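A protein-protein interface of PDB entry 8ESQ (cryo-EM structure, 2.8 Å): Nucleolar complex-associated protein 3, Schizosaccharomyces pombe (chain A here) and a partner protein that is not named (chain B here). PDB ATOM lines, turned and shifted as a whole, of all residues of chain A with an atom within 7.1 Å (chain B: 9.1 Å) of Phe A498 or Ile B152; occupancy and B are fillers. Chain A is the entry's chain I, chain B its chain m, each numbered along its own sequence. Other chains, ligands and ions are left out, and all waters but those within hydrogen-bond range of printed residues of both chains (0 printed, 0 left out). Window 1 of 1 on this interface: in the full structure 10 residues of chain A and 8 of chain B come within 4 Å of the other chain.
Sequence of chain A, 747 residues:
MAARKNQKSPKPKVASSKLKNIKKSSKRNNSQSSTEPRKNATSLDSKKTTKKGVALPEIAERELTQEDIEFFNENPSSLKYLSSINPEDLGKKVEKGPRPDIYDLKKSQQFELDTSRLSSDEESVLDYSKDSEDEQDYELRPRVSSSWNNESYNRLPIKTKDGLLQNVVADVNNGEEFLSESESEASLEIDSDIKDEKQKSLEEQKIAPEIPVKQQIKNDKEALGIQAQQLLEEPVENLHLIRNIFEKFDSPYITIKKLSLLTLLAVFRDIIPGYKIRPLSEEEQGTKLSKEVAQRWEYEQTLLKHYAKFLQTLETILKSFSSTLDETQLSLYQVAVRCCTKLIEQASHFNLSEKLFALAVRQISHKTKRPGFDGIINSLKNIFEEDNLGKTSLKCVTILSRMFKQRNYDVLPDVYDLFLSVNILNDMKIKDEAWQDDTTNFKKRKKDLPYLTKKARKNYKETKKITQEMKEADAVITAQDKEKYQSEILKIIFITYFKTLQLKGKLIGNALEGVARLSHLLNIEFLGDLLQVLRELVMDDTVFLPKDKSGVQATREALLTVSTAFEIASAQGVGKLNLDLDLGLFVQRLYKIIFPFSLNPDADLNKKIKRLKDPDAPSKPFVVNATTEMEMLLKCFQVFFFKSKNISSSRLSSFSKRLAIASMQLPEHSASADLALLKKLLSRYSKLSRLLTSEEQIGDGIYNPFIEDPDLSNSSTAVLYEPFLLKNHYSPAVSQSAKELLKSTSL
Of the printed residues of chain B, Lys A491 touches Ile B155. Phe A498 touches three residues of chain B. No residue of chain B comes within 4 Å of Lys A499. Printed residues of chain B within 4 Å of Gln A502: Leu B148, Asp B149 and Ile B152. Ile B152 touches just these residues of chain A: Ile A495, Phe A498 and Gln A502.
CE of Lys A491 touches O of Ile B155, 3.2 Å away. Ile B155 touches Ile A495 (CG2 to CD1, 3.7 Å). Ile A495 touches Asp B156 (CD1 to OD1, 3.4 Å). Phe A498 touches Leu B148 (O to CD2, 3.7 Å). Ile B152 touches Phe A498 (CG1 to CB, 3.6 Å). CE2 of Phe A498 touches CG1 of Ile B155, at 3.8 Å. CD1 of Leu B148 touches N of Gln A502, at 3.4 Å. Gln A502 touches Ile B152 (OE1 to CD1, 3.7 Å). Phe A526 touches Ser B154 (CE1 to OG, 3.3 Å). Phe A526 touches Ile B155 (CE2 to CD1, 3.5 Å).
The backbone carbonyl oxygen of Ile B152 sits close to the side-chain carboxylate of Asp B156 (2.6 Å). The side-chain amino group (NZ) of Lys A504 sits at hydrogen-bond distance from the backbone carbonyl oxygen (O) of Gln A502, 3.1 Å away.
Hydrophobic or aromatic side chains of chain A that line the printed part of chain B: Ile A495, Phe A498, Leu A501, Phe A526 and Val A533. Among the printed residues, no Asp or Glu carboxylate lies within 4 Å of a Lys or Arg side-chain nitrogen of the other chain.
OE1 of Gln A502 lies close to OD1 of Asp B149, at 3.4 Å.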
ATOM      1  N   TYR A 409     -35.834  -8.101  29.685  1.00  0.00           N
ATOM      2  CA  TYR A 409     -36.613  -8.629  28.564  1.00  0.00           C
ATOM      3  C   TYR A 409     -37.961  -9.175  29.031  1.00  0.00           C
ATOM      4  O   TYR A 409     -38.436 -10.206  28.551  1.00  0.00           O
ATOM      5  CB  TYR A 409     -35.825  -9.693  27.798  1.00  0.00           C
ATOM      6  CG  TYR A 409     -34.503  -9.192  27.264  1.00  0.00           C
ATOM      7  CD1 TYR A 409     -34.416  -8.618  26.003  1.00  0.00           C
ATOM      8  CD2 TYR A 409     -33.344  -9.287  28.022  1.00  0.00           C
ATOM      9  CE1 TYR A 409     -33.212  -8.156  25.511  1.00  0.00           C
ATOM     10  CE2 TYR A 409     -32.135  -8.827  27.539  1.00  0.00           C
ATOM     11  CZ  TYR A 409     -32.075  -8.262  26.283  1.00  0.00           C
ATOM     12  OH  TYR A 409     -30.874  -7.805  25.794  1.00  0.00           O
ATOM     13  N   LEU A 490     -31.283  -5.146  12.535  1.00  0.00           N
ATOM     14  CA  LEU A 490     -31.291  -6.598  12.689  1.00  0.00           C
ATOM     15  C   LEU A 490     -30.380  -7.035  13.826  1.00  0.00           C
ATOM     16  O   LEU A 490     -30.706  -7.967  14.570  1.00  0.00           O
ATOM     17  CB  LEU A 490     -30.873  -7.271  11.382  1.00  0.00           C
ATOM     18  CG  LEU A 490     -31.853  -7.176  10.215  1.00  0.00           C
ATOM     19  CD1 LEU A 490     -31.371  -8.014   9.045  1.00  0.00           C
ATOM     20  CD2 LEU A 490     -33.234  -7.624  10.657  1.00  0.00           C
ATOM     21  N   LYS A 491     -29.228  -6.378  13.971  1.00  0.00           N
ATOM     22  CA  LYS A 491     -28.307  -6.714  15.052  1.00  0.00           C
ATOM     23  C   LYS A 491     -28.954  -6.505  16.415  1.00  0.00           C
ATOM     24  O   LYS A 491     -28.878  -7.372  17.292  1.00  0.00           O
ATOM     25  CB  LYS A 491     -27.035  -5.876  14.925  1.00  0.00           C
ATOM     26  CG  LYS A 491     -25.876  -6.355  15.775  1.00  0.00           C
ATOM     27  CD  LYS A 491     -24.582  -5.689  15.342  1.00  0.00           C
ATOM     28  CE  LYS A 491     -23.377  -6.325  16.009  1.00  0.00           C
ATOM     29  NZ  LYS A 491     -22.100  -5.815  15.440  1.00  0.00           N
ATOM     30  N   ILE A 493     -32.253  -6.089  17.109  1.00  0.00           N
ATOM     31  CA  ILE A 493     -33.487  -6.852  17.270  1.00  0.00           C
ATOM     32  C   ILE A 493     -33.183  -8.315  17.567  1.00  0.00           C
ATOM     33  O   ILE A 493     -33.751  -8.907  18.492  1.00  0.00           O
ATOM     34  CB  ILE A 493     -34.375  -6.700  16.023  1.00  0.00           C
ATOM     35  CG1 ILE A 493     -35.070  -5.339  16.028  1.00  0.00           C
ATOM     36  CG2 ILE A 493     -35.395  -7.814  15.956  1.00  0.00           C
ATOM     37  CD1 ILE A 493     -36.019  -5.141  14.871  1.00  0.00           C
ATOM     38  N   PHE A 494     -32.278  -8.920  16.794  1.00  0.00           N
ATOM     39  CA  PHE A 494     -31.982 -10.336  16.984  1.00  0.00           C
ATOM     40  C   PHE A 494     -31.296 -10.588  18.320  1.00  0.00           C
ATOM     41  O   PHE A 494     -31.539 -11.618  18.961  1.00  0.00           O
ATOM     42  CB  PHE A 494     -31.123 -10.856  15.833  1.00  0.00           C
ATOM     43  CG  PHE A 494     -31.918 -11.464  14.719  1.00  0.00           C
ATOM     44  CD1 PHE A 494     -32.599 -10.664  13.819  1.00  0.00           C
ATOM     45  CD2 PHE A 494     -31.993 -12.838  14.576  1.00  0.00           C
ATOM     46  CE1 PHE A 494     -33.333 -11.222  12.792  1.00  0.00           C
ATOM     47  CE2 PHE A 494     -32.727 -13.403  13.554  1.00  0.00           C
ATOM     48  CZ  PHE A 494     -33.398 -12.594  12.660  1.00  0.00           C
ATOM     49  N   ILE A 495     -30.433  -9.669  18.755  1.00  0.00           N
ATOM     50  CA  ILE A 495     -29.763  -9.848  20.040  1.00  0.00           C
ATOM     51  C   ILE A 495     -30.773  -9.768  21.178  1.00  0.00           C
ATOM     52  O   ILE A 495     -30.615 -10.429  22.211  1.00  0.00           O
ATOM     53  CB  ILE A 495     -28.614  -8.832  20.203  1.00  0.00           C
ATOM     54  CG1 ILE A 495     -27.496  -9.436  21.050  1.00  0.00           C
ATOM     55  CG2 ILE A 495     -29.094  -7.529  20.825  1.00  0.00           C
ATOM     56  CD1 ILE A 495     -26.899 -10.686  20.458  1.00  0.00           C
ATOM     57  N   THR A 496     -31.826  -8.965  21.011  1.00  0.00           N
ATOM     58  CA  THR A 496     -32.884  -8.929  22.014  1.00  0.00           C
ATOM     59  C   THR A 496     -33.699 -10.215  21.995  1.00  0.00           C
ATOM     60  O   THR A 496     -34.063 -10.744  23.052  1.00  0.00           O
ATOM     61  CB  THR A 496     -33.790  -7.720  21.789  1.00  0.00           C
ATOM     62  OG1 THR A 496     -34.128  -7.624  20.400  1.00  0.00           O
ATOM     63  CG2 THR A 496     -33.090  -6.444  22.225  1.00  0.00           C
ATOM     64  N   TYR A 497     -34.002 -10.729  20.801  1.00  0.00           N
ATOM     65  CA  TYR A 497     -34.769 -11.966  20.703  1.00  0.00           C
ATOM     66  C   TYR A 497     -33.998 -13.144  21.283  1.00  0.00           C
ATOM     67  O   TYR A 497     -34.556 -13.949  22.036  1.00  0.00           O
ATOM     68  CB  TYR A 497     -35.141 -12.239  19.246  1.00  0.00           C
ATOM     69  CG  TYR A 497     -36.212 -11.320  18.709  1.00  0.00           C
ATOM     70  CD1 TYR A 497     -36.937 -10.496  19.559  1.00  0.00           C
ATOM     71  CD2 TYR A 497     -36.499 -11.277  17.354  1.00  0.00           C
ATOM     72  CE1 TYR A 497     -37.916  -9.654  19.073  1.00  0.00           C
ATOM     73  CE2 TYR A 497     -37.477 -10.439  16.860  1.00  0.00           C
ATOM     74  CZ  TYR A 497     -38.183  -9.630  17.723  1.00  0.00           C
ATOM     75  OH  TYR A 497     -39.158  -8.792  17.236  1.00  0.00           O
ATOM     76  N   PHE A 498     -32.711 -13.255  20.951  1.00  0.00           N
ATOM     77  CA  PHE A 498     -31.908 -14.357  21.470  1.00  0.00           C
ATOM     78  C   PHE A 498     -31.747 -14.263  22.982  1.00  0.00           C
ATOM     79  O   PHE A 498     -31.735 -15.287  23.674  1.00  0.00           O
ATOM     80  CB  PHE A 498     -30.546 -14.384  20.780  1.00  0.00           C
ATOM     81  CG  PHE A 498     -30.612 -14.740  19.326  1.00  0.00           C
ATOM     82  CD1 PHE A 498     -31.550 -15.648  18.865  1.00  0.00           C
ATOM     83  CD2 PHE A 498     -29.734 -14.175  18.418  1.00  0.00           C
ATOM     84  CE1 PHE A 498     -31.613 -15.982  17.528  1.00  0.00           C
ATOM     85  CE2 PHE A 498     -29.793 -14.505  17.079  1.00  0.00           C
ATOM     86  CZ  PHE A 498     -30.734 -15.410  16.634  1.00  0.00           C
ATOM     87  N   LYS A 499     -31.614 -13.046  23.514  1.00  0.00           N
ATOM     88  CA  LYS A 499     -31.580 -12.881  24.962  1.00  0.00           C
ATOM     89  C   LYS A 499     -32.893 -13.322  25.594  1.00  0.00           C
ATOM     90  O   LYS A 499     -32.899 -13.949  26.660  1.00  0.00           O
ATOM     91  CB  LYS A 499     -31.274 -11.428  25.323  1.00  0.00           C
ATOM     92  CG  LYS A 499     -29.815 -11.033  25.164  1.00  0.00           C
ATOM     93  CD  LYS A 499     -28.918 -11.793  26.123  1.00  0.00           C
ATOM     94  CE  LYS A 499     -27.477 -11.330  26.002  1.00  0.00           C
ATOM     95  NZ  LYS A 499     -26.570 -12.079  26.913  1.00  0.00           N
ATOM     96  N   THR A 500     -34.018 -13.000  24.952  1.00  0.00           N
ATOM     97  CA  THR A 500     -35.313 -13.440  25.462  1.00  0.00           C
ATOM     98  C   THR A 500     -35.412 -14.960  25.468  1.00  0.00           C
ATOM     99  O   THR A 500     -35.930 -15.554  26.421  1.00  0.00           O
ATOM    100  CB  THR A 500     -36.441 -12.834  24.627  1.00  0.00           C
ATOM    101  OG1 THR A 500     -36.329 -11.406  24.632  1.00  0.00           O
ATOM    102  CG2 THR A 500     -37.794 -13.231  25.193  1.00  0.00           C
ATOM    103  N   LEU A 501     -34.916 -15.608  24.412  1.00  0.00           N
ATOM    104  CA  LEU A 501     -34.918 -17.066  24.371  1.00  0.00           C
ATOM    105  C   LEU A 501     -34.056 -17.651  25.481  1.00  0.00           C
ATOM    106  O   LEU A 501     -34.406 -18.681  26.068  1.00  0.00           O
ATOM    107  CB  LEU A 501     -34.439 -17.556  23.005  1.00  0.00           C
ATOM    108  CG  LEU A 501     -35.243 -17.080  21.797  1.00  0.00           C
ATOM    109  CD1 LEU A 501     -34.805 -17.804  20.536  1.00  0.00           C
ATOM    110  CD2 LEU A 501     -36.721 -17.287  22.051  1.00  0.00           C
ATOM    111  N   GLN A 502     -32.919 -17.018  25.773  1.00  0.00           N
ATOM    112  CA  GLN A 502     -32.045 -17.524  26.829  1.00  0.00           C
ATOM    113  C   GLN A 502     -32.735 -17.481  28.185  1.00  0.00           C
ATOM    114  O   GLN A 502     -32.654 -18.438  28.962  1.00  0.00           O
ATOM    115  CB  GLN A 502     -30.747 -16.722  26.866  1.00  0.00           C
ATOM    116  CG  GLN A 502     -29.757 -17.186  27.921  1.00  0.00           C
ATOM    117  CD  GLN A 502     -28.514 -16.324  27.971  1.00  0.00           C
ATOM    118  OE1 GLN A 502     -28.164 -15.662  26.995  1.00  0.00           O
ATOM    119  NE2 GLN A 502     -27.834 -16.332  29.111  1.00  0.00           N
ATOM    120  N   LEU A 503     -33.421 -16.377  28.487  1.00  0.00           N
ATOM    121  CA  LEU A 503     -34.118 -16.262  29.762  1.00  0.00           C
ATOM    122  C   LEU A 503     -35.295 -17.224  29.861  1.00  0.00           C
ATOM    123  O   LEU A 503     -35.706 -17.565  30.976  1.00  0.00           O
ATOM    124  CB  LEU A 503     -34.594 -14.824  29.979  1.00  0.00           C
ATOM    125  CG  LEU A 503     -33.618 -13.842  30.635  1.00  0.00           C
ATOM    126  CD1 LEU A 503     -33.288 -14.287  32.053  1.00  0.00           C
ATOM    127  CD2 LEU A 503     -32.345 -13.661  29.819  1.00  0.00           C
ATOM    128  N   LYS A 504     -35.835 -17.667  28.726  1.00  0.00           N
ATOM    129  CA  LYS A 504     -36.940 -18.624  28.686  1.00  0.00           C
ATOM    130  C   LYS A 504     -38.129 -18.137  29.512  1.00  0.00           C
ATOM    131  O   LYS A 504     -38.699 -18.866  30.327  1.00  0.00           O
ATOM    132  CB  LYS A 504     -36.481 -20.010  29.145  1.00  0.00           C
ATOM    133  CG  LYS A 504     -35.639 -20.748  28.118  1.00  0.00           C
ATOM    134  CD  LYS A 504     -35.358 -22.176  28.547  1.00  0.00           C
ATOM    135  CE  LYS A 504     -34.541 -22.212  29.827  1.00  0.00           C
ATOM    136  NZ  LYS A 504     -33.317 -21.372  29.723  1.00  0.00           N
ATOM    137  N   ALA A 511     -40.893 -13.607  20.607  1.00  0.00           N
ATOM    138  CA  ALA A 511     -39.538 -13.761  20.087  1.00  0.00           C
ATOM    139  C   ALA A 511     -39.524 -14.649  18.848  1.00  0.00           C
ATOM    140  O   ALA A 511     -38.905 -14.309  17.833  1.00  0.00           O
ATOM    141  CB  ALA A 511     -38.623 -14.329  21.170  1.00  0.00           C
ATOM    142  N   VAL A 515     -38.507 -13.794  15.026  1.00  0.00           N
ATOM    143  CA  VAL A 515     -37.465 -14.594  14.384  1.00  0.00           C
ATOM    144  C   VAL A 515     -37.969 -15.157  13.062  1.00  0.00           C
ATOM    145  O   VAL A 515     -37.271 -15.113  12.042  1.00  0.00           O
ATOM    146  CB  VAL A 515     -36.984 -15.709  15.329  1.00  0.00           C
ATOM    147  CG1 VAL A 515     -36.184 -16.747  14.561  1.00  0.00           C
ATOM    148  CG2 VAL A 515     -36.145 -15.124  16.451  1.00  0.00           C
ATOM    149  N   LEU A 522     -31.773 -12.351   7.307  1.00  0.00           N
ATOM    150  CA  LEU A 522     -30.462 -12.629   7.866  1.00  0.00           C
ATOM    151  C   LEU A 522     -29.596 -13.405   6.875  1.00  0.00           C
ATOM    152  O   LEU A 522     -30.058 -13.871   5.830  1.00  0.00           O
ATOM    153  CB  LEU A 522     -30.602 -13.401   9.176  1.00  0.00           C
ATOM    154  CG  LEU A 522     -29.615 -13.017  10.275  1.00  0.00           C
ATOM    155  CD1 LEU A 522     -29.713 -11.531  10.562  1.00  0.00           C
ATOM    156  CD2 LEU A 522     -29.879 -13.823  11.533  1.00  0.00           C
ATOM    157  N   PHE A 526     -26.333 -17.956   9.118  1.00  0.00           N
ATOM    158  CA  PHE A 526     -27.141 -17.913  10.328  1.00  0.00           C
ATOM    159  C   PHE A 526     -28.390 -18.778  10.221  1.00  0.00           C
ATOM    160  O   PHE A 526     -28.902 -19.227  11.251  1.00  0.00           O
ATOM    161  CB  PHE A 526     -27.519 -16.468  10.648  1.00  0.00           C
ATOM    162  CG  PHE A 526     -26.373 -15.648  11.163  1.00  0.00           C
ATOM    163  CD1 PHE A 526     -25.279 -16.261  11.749  1.00  0.00           C
ATOM    164  CD2 PHE A 526     -26.380 -14.269  11.048  1.00  0.00           C
ATOM    165  CE1 PHE A 526     -24.220 -15.514  12.220  1.00  0.00           C
ATOM    166  CE2 PHE A 526     -25.322 -13.517  11.516  1.00  0.00           C
ATOM    167  CZ  PHE A 526     -24.241 -14.140  12.105  1.00  0.00           C
ATOM    168  N   ASP A 529     -27.551 -22.222  11.637  1.00  0.00           N
ATOM    169  CA  ASP A 529     -27.432 -22.208  13.087  1.00  0.00           C
ATOM    170  C   ASP A 529     -28.704 -21.739  13.782  1.00  0.00           C
ATOM    171  O   ASP A 529     -28.801 -21.868  15.006  1.00  0.00           O
ATOM    172  CB  ASP A 529     -26.256 -21.324  13.506  1.00  0.00           C
ATOM    173  CG  ASP A 529     -24.916 -21.908  13.099  1.00  0.00           C
ATOM    174  OD1 ASP A 529     -24.546 -22.976  13.629  1.00  0.00           O
ATOM    175  OD2 ASP A 529     -24.236 -21.299  12.248  1.00  0.00           O
ATOM    176  N   LEU A 530     -29.673 -21.202  13.037  1.00  0.00           N
ATOM    177  CA  LEU A 530     -30.912 -20.746  13.659  1.00  0.00           C
ATOM    178  C   LEU A 530     -31.730 -21.913  14.196  1.00  0.00           C
ATOM    179  O   LEU A 530     -32.387 -21.791  15.233  1.00  0.00           O
ATOM    180  CB  LEU A 530     -31.736 -19.930  12.664  1.00  0.00           C
ATOM    181  CG  LEU A 530     -31.570 -18.414  12.757  1.00  0.00           C
ATOM    182  CD1 LEU A 530     -32.339 -17.717  11.647  1.00  0.00           C
ATOM    183  CD2 LEU A 530     -32.013 -17.914  14.123  1.00  0.00           C
ATOM    184  N   VAL A 533     -30.779 -23.443  17.957  1.00  0.00           N
ATOM    185  CA  VAL A 533     -31.362 -22.876  19.171  1.00  0.00           C
ATOM    186  C   VAL A 533     -32.811 -23.324  19.326  1.00  0.00           C
ATOM    187  O   VAL A 533     -33.300 -23.518  20.445  1.00  0.00           O
ATOM    188  CB  VAL A 533     -31.225 -21.340  19.177  1.00  0.00           C
ATOM    189  CG1 VAL A 533     -31.967 -20.714  18.019  1.00  0.00           C
ATOM    190  CG2 VAL A 533     -31.733 -20.771  20.485  1.00  0.00           C
ATOM    191  N   PRO B 145     -20.449 -24.836  23.279  1.00  0.00           N
ATOM    192  CA  PRO B 145     -21.308 -23.865  23.969  1.00  0.00           C
ATOM    193  C   PRO B 145     -22.750 -23.899  23.485  1.00  0.00           C
ATOM    194  O   PRO B 145     -23.008 -24.356  22.370  1.00  0.00           O
ATOM    195  CB  PRO B 145     -20.679 -22.520  23.594  1.00  0.00           C
ATOM    196  CG  PRO B 145     -19.973 -22.782  22.307  1.00  0.00           C
ATOM    197  CD  PRO B 145     -19.435 -24.176  22.440  1.00  0.00           C
ATOM    198  N   ALA B 146     -23.676 -23.415  24.306  1.00  0.00           N
ATOM    199  CA  ALA B 146     -25.078 -23.368  23.905  1.00  0.00           C
ATOM    200  C   ALA B 146     -25.198 -22.685  22.559  1.00  0.00           C
ATOM    201  O   ALA B 146     -24.660 -21.598  22.360  1.00  0.00           O
ATOM    202  CB  ALA B 146     -25.908 -22.637  24.944  1.00  0.00           C
ATOM    203  N   ALA B 147     -25.900 -23.319  21.629  1.00  0.00           N
ATOM    204  CA  ALA B 147     -25.992 -22.752  20.289  1.00  0.00           C
ATOM    205  C   ALA B 147     -26.630 -21.375  20.327  1.00  0.00           C
ATOM    206  O   ALA B 147     -26.354 -20.528  19.471  1.00  0.00           O
ATOM    207  CB  ALA B 147     -26.779 -23.686  19.372  1.00  0.00           C
ATOM    208  N   LEU B 148     -27.492 -21.137  21.313  1.00  0.00           N
ATOM    209  CA  LEU B 148     -27.983 -19.789  21.564  1.00  0.00           C
ATOM    210  C   LEU B 148     -26.838 -18.856  21.941  1.00  0.00           C
ATOM    211  O   LEU B 148     -26.681 -17.777  21.356  1.00  0.00           O
ATOM    212  CB  LEU B 148     -29.040 -19.831  22.666  1.00  0.00           C
ATOM    213  CG  LEU B 148     -29.823 -18.572  23.014  1.00  0.00           C
ATOM    214  CD1 LEU B 148     -31.196 -18.949  23.524  1.00  0.00           C
ATOM    215  CD2 LEU B 148     -29.078 -17.795  24.069  1.00  0.00           C
ATOM    216  N   ASP B 149     -26.027 -19.256  22.925  1.00  0.00           N
ATOM    217  CA  ASP B 149     -24.950 -18.393  23.401  1.00  0.00           C
ATOM    218  C   ASP B 149     -23.903 -18.161  22.320  1.00  0.00           C
ATOM    219  O   ASP B 149     -23.413 -17.037  22.154  1.00  0.00           O
ATOM    220  CB  ASP B 149     -24.308 -18.993  24.649  1.00  0.00           C
ATOM    221  CG  ASP B 149     -25.267 -19.067  25.818  1.00  0.00           C
ATOM    222  OD1 ASP B 149     -26.155 -18.193  25.916  1.00  0.00           O
ATOM    223  OD2 ASP B 149     -25.138 -20.000  26.637  1.00  0.00           O
ATOM    224  N   SER B 150     -23.540 -19.211  21.580  1.00  0.00           N
ATOM    225  CA  SER B 150     -22.594 -19.045  20.483  1.00  0.00           C
ATOM    226  C   SER B 150     -23.164 -18.133  19.406  1.00  0.00           C
ATOM    227  O   SER B 150     -22.444 -17.301  18.842  1.00  0.00           O
ATOM    228  CB  SER B 150     -22.223 -20.406  19.896  1.00  0.00           C
ATOM    229  OG  SER B 150     -23.146 -20.799  18.895  1.00  0.00           O
ATOM    230  N   LEU B 151     -24.455 -18.278  19.104  1.00  0.00           N
ATOM    231  CA  LEU B 151     -25.083 -17.401  18.121  1.00  0.00           C
ATOM    232  C   LEU B 151     -25.110 -15.959  18.606  1.00  0.00           C
ATOM    233  O   LEU B 151     -24.906 -15.033  17.815  1.00  0.00           O
ATOM    234  CB  LEU B 151     -26.495 -17.888  17.803  1.00  0.00           C
ATOM    235  CG  LEU B 151     -26.949 -17.758  16.348  1.00  0.00           C
ATOM    236  CD1 LEU B 151     -25.764 -17.845  15.398  1.00  0.00           C
ATOM    237  CD2 LEU B 151     -27.981 -18.823  16.015  1.00  0.00           C
ATOM    238  N   ILE B 152     -25.360 -15.748  19.902  1.00  0.00           N
ATOM    239  CA  ILE B 152     -25.323 -14.393  20.448  1.00  0.00           C
ATOM    240  C   ILE B 152     -23.945 -13.778  20.252  1.00  0.00           C
ATOM    241  O   ILE B 152     -23.817 -12.664  19.729  1.00  0.00           O
ATOM    242  CB  ILE B 152     -25.732 -14.390  21.931  1.00  0.00           C
ATOM    243  CG1 ILE B 152     -27.242 -14.565  22.071  1.00  0.00           C
ATOM    244  CG2 ILE B 152     -25.266 -13.116  22.617  1.00  0.00           C
ATOM    245  CD1 ILE B 152     -27.709 -14.627  23.502  1.00  0.00           C
ATOM    246  N   ALA B 153     -22.893 -14.503  20.640  1.00  0.00           N
ATOM    247  CA  ALA B 153     -21.541 -13.973  20.504  1.00  0.00           C
ATOM    248  C   ALA B 153     -21.217 -13.663  19.049  1.00  0.00           C
ATOM    249  O   ALA B 153     -20.577 -12.648  18.750  1.00  0.00           O
ATOM    250  CB  ALA B 153     -20.528 -14.959  21.084  1.00  0.00           C
ATOM    251  N   SER B 154     -21.649 -14.528  18.129  1.00  0.00           N
ATOM    252  CA  SER B 154     -21.459 -14.246  16.711  1.00  0.00           C
ATOM    253  C   SER B 154     -22.264 -13.026  16.275  1.00  0.00           C
ATOM    254  O   SER B 154     -21.788 -12.218  15.469  1.00  0.00           O
ATOM    255  CB  SER B 154     -21.842 -15.468  15.877  1.00  0.00           C
ATOM    256  OG  SER B 154     -21.906 -15.143  14.499  1.00  0.00           O
ATOM    257  N   ILE B 155     -23.490 -12.882  16.784  1.00  0.00           N
ATOM    258  CA  ILE B 155     -24.322 -11.745  16.396  1.00  0.00           C
ATOM    259  C   ILE B 155     -23.707 -10.441  16.891  1.00  0.00           C
ATOM    260  O   ILE B 155     -23.525  -9.491  16.122  1.00  0.00           O
ATOM    261  CB  ILE B 155     -25.761 -11.922  16.913  1.00  0.00           C
ATOM    262  CG1 ILE B 155     -26.489 -13.005  16.116  1.00  0.00           C
ATOM    263  CG2 ILE B 155     -26.519 -10.608  16.827  1.00  0.00           C
ATOM    264  CD1 ILE B 155     -26.659 -12.680  14.655  1.00  0.00           C
ATOM    265  N   ASP B 156     -23.367 -10.380  18.177  1.00  0.00           N
ATOM    266  CA  ASP B 156     -22.727  -9.202  18.763  1.00  0.00           C
ATOM    267  C   ASP B 156     -21.344  -9.595  19.283  1.00  0.00           C
ATOM    268  O   ASP B 156     -21.178 -10.141  20.375  1.00  0.00           O
ATOM    269  CB  ASP B 156     -23.667  -8.500  19.882  1.00  0.00           C
ATOM    270  CG  ASP B 156     -23.735  -9.262  21.200  1.00  0.00           C
ATOM    271  OD1 ASP B 156     -23.549 -10.493  21.213  1.00  0.00           O
ATOM    272  OD2 ASP B 156     -24.050  -8.626  22.228  1.00  0.00           O
ATOM    273  N   LYS B 157     -20.332  -9.331  18.458  1.00  0.00           N
ATOM    274  CA  LYS B 157     -18.954  -9.619  18.828  1.00  0.00           C
ATOM    275  C   LYS B 157     -18.579  -8.870  20.098  1.00  0.00           C
ATOM    276  O   LYS B 157     -18.911  -7.694  20.264  1.00  0.00           O
ATOM    277  CB  LYS B 157     -18.016  -9.228  17.686  1.00  0.00           C
ATOM    278  CG  LYS B 157     -18.396  -9.843  16.356  1.00  0.00           C
ATOM    279  CD  LYS B 157     -18.315 -11.356  16.405  1.00  0.00           C
ATOM    280  CE  LYS B 157     -18.580 -11.954  15.038  1.00  0.00           C
ATOM    281  NZ  LYS B 157     -18.148 -11.035  13.952  1.00  0.00           N
ATOM    282  N   ASP B 158     -17.891  -9.565  20.996  1.00  0.00           N
ATOM    283  CA  ASP B 158     -17.450  -8.948  22.236  1.00  0.00           C
ATOM    284  C   ASP B 158     -16.443  -7.846  21.937  1.00  0.00           C
ATOM    285  O   ASP B 158     -15.727  -7.882  20.933  1.00  0.00           O
ATOM    286  CB  ASP B 158     -16.828  -9.995  23.160  1.00  0.00           C
ATOM    287  CG  ASP B 158     -16.470  -9.440  24.531  1.00  0.00           C
ATOM    288  OD1 ASP B 158     -16.686  -8.234  24.779  1.00  0.00           O
ATOM    289  OD2 ASP B 158     -15.962 -10.217  25.366  1.00  0.00           O
